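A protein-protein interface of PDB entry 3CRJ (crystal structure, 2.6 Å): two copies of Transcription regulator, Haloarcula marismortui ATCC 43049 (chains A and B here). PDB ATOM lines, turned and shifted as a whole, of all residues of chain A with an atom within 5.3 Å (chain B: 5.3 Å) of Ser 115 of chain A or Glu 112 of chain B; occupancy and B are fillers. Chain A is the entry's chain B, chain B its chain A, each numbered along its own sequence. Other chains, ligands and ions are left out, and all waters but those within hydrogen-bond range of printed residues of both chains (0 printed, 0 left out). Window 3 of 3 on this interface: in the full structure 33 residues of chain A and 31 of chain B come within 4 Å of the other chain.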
ATOM      1  N   LEU A 111      -0.224 -29.508  16.101  1.00  0.00           N
ATOM      2  CA  LEU A 111      -0.539 -28.304  15.332  1.00  0.00           C
ATOM      3  C   LEU A 111      -0.320 -27.073  16.198  1.00  0.00           C
ATOM      4  O   LEU A 111       0.195 -26.058  15.728  1.00  0.00           O
ATOM      5  CB  LEU A 111      -1.975 -28.318  14.805  1.00  0.00           C
ATOM      6  CG  LEU A 111      -2.344 -27.737  13.416  1.00  0.00           C
ATOM      7  CD1 LEU A 111      -3.783 -27.189  13.384  1.00  0.00           C
ATOM      8  CD2 LEU A 111      -1.405 -26.689  12.866  1.00  0.00           C
ATOM      9  N   GLU A 112      -0.694 -27.161  17.470  1.00  0.00           N
ATOM     10  CA  GLU A 112      -0.507 -26.009  18.356  1.00  0.00           C
ATOM     11  C   GLU A 112       0.971 -25.591  18.467  1.00  0.00           C
ATOM     12  O   GLU A 112       1.273 -24.406  18.337  1.00  0.00           O
ATOM     13  CB  GLU A 112      -1.129 -26.235  19.721  1.00  0.00           C
ATOM     14  CG  GLU A 112      -2.621 -26.462  19.724  1.00  0.00           C
ATOM     15  CD  GLU A 112      -3.121 -26.674  21.129  1.00  0.00           C
ATOM     16  OE1 GLU A 112      -3.287 -27.841  21.530  1.00  0.00           O
ATOM     17  OE2 GLU A 112      -3.297 -25.677  21.862  1.00  0.00           O
ATOM     18  N   MET A 113       1.876 -26.559  18.658  1.00  0.00           N
ATOM     19  CA  MET A 113       3.319 -26.291  18.670  1.00  0.00           C
ATOM     20  C   MET A 113       3.734 -25.638  17.367  1.00  0.00           C
ATOM     21  O   MET A 113       4.541 -24.712  17.363  1.00  0.00           O
ATOM     22  CB  MET A 113       4.175 -27.560  18.807  1.00  0.00           C
ATOM     23  CG  MET A 113       3.585 -28.720  19.537  1.00  0.00           C
ATOM     24  SD  MET A 113       4.262 -28.903  21.343  1.00  0.00           S
ATOM     25  CE  MET A 113       4.755 -30.779  21.176  1.00  0.00           C
ATOM     26  N   ARG A 114       3.214 -26.132  16.252  1.00  0.00           N
ATOM     27  CA  ARG A 114       3.613 -25.559  14.987  1.00  0.00           C
ATOM     28  C   ARG A 114       3.248 -24.087  14.923  1.00  0.00           C
ATOM     29  O   ARG A 114       4.059 -23.269  14.499  1.00  0.00           O
ATOM     30  CB  ARG A 114       2.988 -26.289  13.827  1.00  0.00           C
ATOM     31  CG  ARG A 114       3.848 -27.383  13.268  1.00  0.00           C
ATOM     32  CD  ARG A 114       3.227 -27.819  11.966  1.00  0.00           C
ATOM     33  NE  ARG A 114       4.033 -28.787  11.239  1.00  0.00           N
ATOM     34  CZ  ARG A 114       4.086 -30.085  11.521  1.00  0.00           C
ATOM     35  NH1 ARG A 114       3.391 -30.594  12.547  1.00  0.00           N
ATOM     36  NH2 ARG A 114       4.846 -30.876  10.770  1.00  0.00           N
ATOM     37  N   SER A 115       2.046 -23.751  15.376  1.00  0.00           N
ATOM     38  CA  SER A 115       1.606 -22.366  15.400  1.00  0.00           C
ATOM     39  C   SER A 115       2.472 -21.478  16.313  1.00  0.00           C
ATOM     40  O   SER A 115       2.438 -20.265  16.203  1.00  0.00           O
ATOM     41  CB  SER A 115       0.117 -22.290  15.768  1.00  0.00           C
ATOM     42  OG  SER A 115      -0.108 -22.472  17.154  1.00  0.00           O
ATOM     43  N   GLN A 116       3.243 -22.093  17.203  1.00  0.00           N
ATOM     44  CA  GLN A 116       4.160 -21.380  18.093  1.00  0.00           C
ATOM     45  C   GLN A 116       5.537 -21.198  17.493  1.00  0.00           C
ATOM     46  O   GLN A 116       6.278 -20.333  17.907  1.00  0.00           O
ATOM     47  CB  GLN A 116       4.303 -22.111  19.421  1.00  0.00           C
ATOM     48  CG  GLN A 116       3.133 -21.995  20.316  1.00  0.00           C
ATOM     49  CD  GLN A 116       2.582 -20.606  20.321  1.00  0.00           C
ATOM     50  OE1 GLN A 116       1.760 -20.244  19.474  1.00  0.00           O
ATOM     51  NE2 GLN A 116       3.037 -19.799  21.268  1.00  0.00           N
ATOM     52  N   ALA A 117       5.878 -22.026  16.518  1.00  0.00           N
ATOM     53  CA  ALA A 117       7.164 -21.921  15.798  1.00  0.00           C
ATOM     54  C   ALA A 117       7.599 -20.471  15.514  1.00  0.00           C
ATOM     55  O   ALA A 117       8.742 -20.114  15.789  1.00  0.00           O
ATOM     56  CB  ALA A 117       7.114 -22.732  14.512  1.00  0.00           C
ATOM     57  N   PRO A 118       6.680 -19.620  15.010  1.00  0.00           N
ATOM     58  CA  PRO A 118       7.040 -18.216  14.833  1.00  0.00           C
ATOM     59  C   PRO A 118       7.263 -17.475  16.133  1.00  0.00           C
ATOM     60  O   PRO A 118       7.754 -16.371  16.094  1.00  0.00           O
ATOM     61  CB  PRO A 118       5.807 -17.614  14.141  1.00  0.00           C
ATOM     62  CG  PRO A 118       5.025 -18.771  13.642  1.00  0.00           C
ATOM     63  CD  PRO A 118       5.288 -19.871  14.602  1.00  0.00           C
ATOM     64  N   TYR A 119       6.892 -18.022  17.277  1.00  0.00           N
ATOM     65  CA  TYR A 119       7.171 -17.294  18.512  1.00  0.00           C
ATOM     66  C   TYR A 119       8.353 -17.835  19.284  1.00  0.00           C
ATOM     67  O   TYR A 119       8.915 -17.110  20.080  1.00  0.00           O
ATOM     68  CB  TYR A 119       5.941 -17.182  19.410  1.00  0.00           C
ATOM     69  CG  TYR A 119       4.832 -16.424  18.743  1.00  0.00           C
ATOM     70  CD1 TYR A 119       4.007 -17.058  17.838  1.00  0.00           C
ATOM     71  CD2 TYR A 119       4.616 -15.068  18.993  1.00  0.00           C
ATOM     72  CE1 TYR A 119       2.984 -16.387  17.199  1.00  0.00           C
ATOM     73  CE2 TYR A 119       3.592 -14.383  18.357  1.00  0.00           C
ATOM     74  CZ  TYR A 119       2.774 -15.053  17.450  1.00  0.00           C
ATOM     75  OH  TYR A 119       1.738 -14.432  16.764  1.00  0.00           O
ATOM     76  N   GLY B  31      -0.269 -10.678  16.718  1.00  0.00           N
ATOM     77  CA  GLY B  31      -0.595 -12.091  16.599  1.00  0.00           C
ATOM     78  C   GLY B  31      -1.886 -12.406  17.328  1.00  0.00           C
ATOM     79  O   GLY B  31      -2.487 -11.535  17.964  1.00  0.00           O
ATOM     80  N   TYR B  32      -2.312 -13.663  17.259  1.00  0.00           N
ATOM     81  CA  TYR B  32      -3.532 -14.056  17.953  1.00  0.00           C
ATOM     82  C   TYR B  32      -3.395 -13.960  19.476  1.00  0.00           C
ATOM     83  O   TYR B  32      -4.164 -13.276  20.114  1.00  0.00           O
ATOM     84  CB  TYR B  32      -4.021 -15.454  17.541  1.00  0.00           C
ATOM     85  CG  TYR B  32      -5.165 -15.898  18.420  1.00  0.00           C
ATOM     86  CD1 TYR B  32      -6.446 -15.377  18.244  1.00  0.00           C
ATOM     87  CD2 TYR B  32      -4.959 -16.798  19.460  1.00  0.00           C
ATOM     88  CE1 TYR B  32      -7.493 -15.749  19.083  1.00  0.00           C
ATOM     89  CE2 TYR B  32      -5.996 -17.168  20.300  1.00  0.00           C
ATOM     90  CZ  TYR B  32      -7.259 -16.641  20.106  1.00  0.00           C
ATOM     91  OH  TYR B  32      -8.291 -17.011  20.939  1.00  0.00           O
ATOM     92  N   ALA B  33      -2.419 -14.641  20.055  1.00  0.00           N
ATOM     93  CA  ALA B  33      -2.341 -14.767  21.517  1.00  0.00           C
ATOM     94  C   ALA B  33      -2.399 -13.429  22.285  1.00  0.00           C
ATOM     95  O   ALA B  33      -2.982 -13.325  23.360  1.00  0.00           O
ATOM     96  CB  ALA B  33      -1.099 -15.552  21.903  1.00  0.00           C
ATOM     97  N   SER B 107      -0.806 -14.365   8.230  1.00  0.00           N
ATOM     98  CA  SER B 107      -0.684 -15.812   8.165  1.00  0.00           C
ATOM     99  C   SER B 107      -0.334 -16.531   9.476  1.00  0.00           C
ATOM    100  O   SER B 107      -0.949 -17.560   9.778  1.00  0.00           O
ATOM    101  CB  SER B 107       0.223 -16.209   7.016  1.00  0.00           C
ATOM    102  OG  SER B 107      -0.501 -15.972   5.815  1.00  0.00           O
ATOM    103  N   VAL B 108       0.614 -15.985  10.248  1.00  0.00           N
ATOM    104  CA  VAL B 108       0.930 -16.486  11.594  1.00  0.00           C
ATOM    105  C   VAL B 108      -0.336 -16.517  12.459  1.00  0.00           C
ATOM    106  O   VAL B 108      -0.679 -17.551  13.030  1.00  0.00           O
ATOM    107  CB  VAL B 108       1.988 -15.598  12.285  1.00  0.00           C
ATOM    108  CG1 VAL B 108       2.107 -15.903  13.779  1.00  0.00           C
ATOM    109  CG2 VAL B 108       3.343 -15.684  11.560  1.00  0.00           C
ATOM    110  N   ALA B 109      -1.045 -15.394  12.512  1.00  0.00           N
ATOM    111  CA  ALA B 109      -2.287 -15.293  13.279  1.00  0.00           C
ATOM    112  C   ALA B 109      -3.310 -16.356  12.911  1.00  0.00           C
ATOM    113  O   ALA B 109      -3.893 -16.979  13.799  1.00  0.00           O
ATOM    114  CB  ALA B 109      -2.895 -13.924  13.133  1.00  0.00           C
ATOM    115  N   LEU B 110      -3.503 -16.570  11.608  1.00  0.00           N
ATOM    116  CA  LEU B 110      -4.487 -17.545  11.121  1.00  0.00           C
ATOM    117  C   LEU B 110      -4.153 -19.021  11.437  1.00  0.00           C
ATOM    118  O   LEU B 110      -5.056 -19.820  11.667  1.00  0.00           O
ATOM    119  CB  LEU B 110      -4.758 -17.351   9.625  1.00  0.00           C
ATOM    120  CG  LEU B 110      -5.405 -16.045   9.114  1.00  0.00           C
ATOM    121  CD1 LEU B 110      -5.335 -16.053   7.601  1.00  0.00           C
ATOM    122  CD2 LEU B 110      -6.826 -15.918   9.527  1.00  0.00           C
ATOM    123  N   LEU B 111      -2.874 -19.377  11.460  1.00  0.00           N
ATOM    124  CA  LEU B 111      -2.466 -20.722  11.860  1.00  0.00           C
ATOM    125  C   LEU B 111      -2.698 -20.915  13.360  1.00  0.00           C
ATOM    126  O   LEU B 111      -3.127 -21.981  13.795  1.00  0.00           O
ATOM    127  CB  LEU B 111      -0.987 -20.956  11.557  1.00  0.00           C
ATOM    128  CG  LEU B 111      -0.401 -22.314  11.114  1.00  0.00           C
ATOM    129  CD1 LEU B 111       0.999 -22.501  11.714  1.00  0.00           C
ATOM    130  CD2 LEU B 111      -1.260 -23.555  11.367  1.00  0.00           C
ATOM    131  N   GLU B 112      -2.427 -19.876  14.143  1.00  0.00           N
ATOM    132  CA  GLU B 112      -2.674 -19.936  15.575  1.00  0.00           C
ATOM    133  C   GLU B 112      -4.148 -20.213  15.775  1.00  0.00           C
ATOM    134  O   GLU B 112      -4.526 -21.083  16.558  1.00  0.00           O
ATOM    135  CB  GLU B 112      -2.312 -18.627  16.282  1.00  0.00           C
ATOM    136  CG  GLU B 112      -0.850 -18.248  16.291  1.00  0.00           C
ATOM    137  CD  GLU B 112      -0.615 -16.916  17.000  1.00  0.00           C
ATOM    138  OE1 GLU B 112      -0.297 -15.921  16.307  1.00  0.00           O
ATOM    139  OE2 GLU B 112      -0.765 -16.846  18.249  1.00  0.00           O
ATOM    140  N   MET B 113      -4.979 -19.475  15.051  1.00  0.00           N
ATOM    141  CA  MET B 113      -6.419 -19.609  15.181  1.00  0.00           C
ATOM    142  C   MET B 113      -6.930 -20.949  14.664  1.00  0.00           C
ATOM    143  O   MET B 113      -7.869 -21.503  15.235  1.00  0.00           O
ATOM    144  CB  MET B 113      -7.121 -18.462  14.474  1.00  0.00           C
ATOM    145  CG  MET B 113      -6.976 -17.147  15.173  1.00  0.00           C
ATOM    146  SD  MET B 113      -7.896 -15.747  14.207  1.00  0.00           S
ATOM    147  CE  MET B 113      -7.647 -16.466  12.419  1.00  0.00           C
ATOM    148  N   ARG B 114      -6.298 -21.471  13.607  1.00  0.00           N
ATOM    149  CA  ARG B 114      -6.638 -22.795  13.077  1.00  0.00           C
ATOM    150  C   ARG B 114      -6.310 -23.885  14.065  1.00  0.00           C
ATOM    151  O   ARG B 114      -7.077 -24.832  14.226  1.00  0.00           O
ATOM    152  CB  ARG B 114      -5.921 -23.094  11.776  1.00  0.00           C
ATOM    153  CG  ARG B 114      -6.585 -22.519  10.565  1.00  0.00           C
ATOM    154  CD  ARG B 114      -5.895 -22.992   9.290  1.00  0.00           C
ATOM    155  NE  ARG B 114      -6.198 -22.139   8.143  1.00  0.00           N
ATOM    156  CZ  ARG B 114      -5.437 -21.108   7.762  1.00  0.00           C
ATOM    157  NH1 ARG B 114      -4.327 -20.795   8.455  1.00  0.00           N
ATOM    158  NH2 ARG B 114      -5.793 -20.382   6.694  1.00  0.00           N
ATOM    159  N   SER B 115      -5.161 -23.751  14.726  1.00  0.00           N
ATOM    160  CA  SER B 115      -4.756 -24.732  15.728  1.00  0.00           C
ATOM    161  C   SER B 115      -5.707 -24.726  16.913  1.00  0.00           C
ATOM    162  O   SER B 115      -5.735 -25.681  17.667  1.00  0.00           O
ATOM    163  CB  SER B 115      -3.298 -24.551  16.155  1.00  0.00           C
ATOM    164  OG  SER B 115      -3.141 -23.472  17.053  1.00  0.00           O
ATOM    165  N   GLN B 116      -6.507 -23.668  17.045  1.00  0.00           N
ATOM    166  CA  GLN B 116      -7.521 -23.586  18.102  1.00  0.00           C
ATOM    167  C   GLN B 116      -8.934 -24.025  17.761  1.00  0.00           C
ATOM    168  O   GLN B 116      -9.768 -24.135  18.639  1.00  0.00           O
ATOM    169  CB  GLN B 116      -7.559 -22.203  18.683  1.00  0.00           C
ATOM    170  CG  GLN B 116      -6.731 -22.121  19.909  1.00  0.00           C
ATOM    171  CD  GLN B 116      -6.358 -20.714  20.193  1.00  0.00           C
ATOM    172  OE1 GLN B 116      -5.987 -19.961  19.277  1.00  0.00           O
ATOM    173  NE2 GLN B 116      -6.451 -20.320  21.467  1.00  0.00           N
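The side-chain hydroxyl (OH) of Tyr 119 of chain A lies within hydrogen-bond range of the side-chain carboxylate (OE1) of Glu 112 of chain B (2.6 Å).
The side-chain hydroxyl (OG) of Ser 115 of chain B lies within hydrogen-bond range of the side-chain hydroxyl (OG) of Ser 115 of chain A, at 3.2 Å.
The side-chain hydroxyl of Ser 115 of chain B is in hydrogen-bond range of the backbone carbonyl oxygen of Glu 112 of chain B (2.8 Å).
The backbone carbonyl oxygen (O) of Glu 112 of chain A is in hydrogen-bond range of the side-chain hydroxyl (OG) of Ser 115 of chain A (2.7 Å).
N of Ala 33 of chain B sits at hydrogen-bond distance from OE2 of Glu 112 of chain B (3.3 Å).
The backbone carbonyl oxygen of Glu 112 of chain B sits close to the side-chain amide oxygen of Gln 116 of chain B (3.3 Å).
N of Tyr 32 of chain B sits at hydrogen-bond distance from OE1 of Glu 112 of chain B (3.2 Å).
Among the printed residues, pairs that only touch across the chains: Leu 111 of chain A with Leu 111 of chain B (3.5 Å), Leu 111 of chain A with Ser 115 of chain B (3.5 Å), Glu 112 of chain A with Ser 115 of chain B (3.8 Å), Ser 115 of chain A with Leu 111 of chain B (3.7 Å), Ser 115 of chain A with Glu 112 of chain B (3.7 Å), Tyr 119 of chain A with Gly 31 of chain B (3.3 Å) and Tyr 119 of chain A with Val 108 of chain B (3.3 Å).
Printed residues of chain B within 4 Å of Leu 111 of chain A: Leu 111 and Ser 115.
Ser 115 of chain A touches just these residues of chain B: Leu 111, Glu 112 and Ser 115.
Of the printed residues of chain B, Tyr 119 of chain A touches Gly 31, Val 108 and Glu 112.
Printed residues of chain A within 4 Å of Gly 31 of chain B: Tyr 119.
Leu 110 of chain B touches none of the printed residues of chain A.
Of the printed residues of chain A, Leu 111 of chain B touches Leu 111 and Ser 115.
Of chain A, only Ser 115 and Tyr 119 come within 4 Å of Glu 112 of chain B.
Of the printed residues of chain A, Ser 115 of chain B touches Leu 111, Glu 112 and Ser 115.
The nearest residue of chain A that does not touch Glu 112 of chain B is Gln 116 of chain A (4.4 Å).
The nearest printed residue of chain B that does not touch Tyr 119 of chain A is Tyr 32 of chain B (4.2 Å).
Hydrophobic or aromatic side chains of chain A within 4 Å of the printed part of chain B: Leu 111 and Tyr 119.
Hydrophobic or aromatic side chains of chain B within 4 Å of the printed part of chain A: Val 108 and Leu 111.
Along chain B the printed residues that touch a printed residue of chain A span positions 31 to 115.
Among the printed residues, 9 pairs touch across the chains.
Leu 111 of chain A touches its own counterpart, Leu 111 of chain B.
Leu 111 of chain A touches Ser 115 of chain B, and with the chains exchanged Ser 115 of chain A touches Leu 111 of chain B.
Glu 112 of chain A touches Ser 115 of chain B, and with the chains exchanged Ser 115 of chain A touches Glu 112 of chain B.
Ser 115 of chain A touches its own counterpart, Ser 115 of chain B.
Positions printed for both chains: 111, 112, 113, 114, 115 and 116.
Of the 9 pairs that touch across the chains among the printed residues, 6 have their exchanged pair printed and touching as well.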
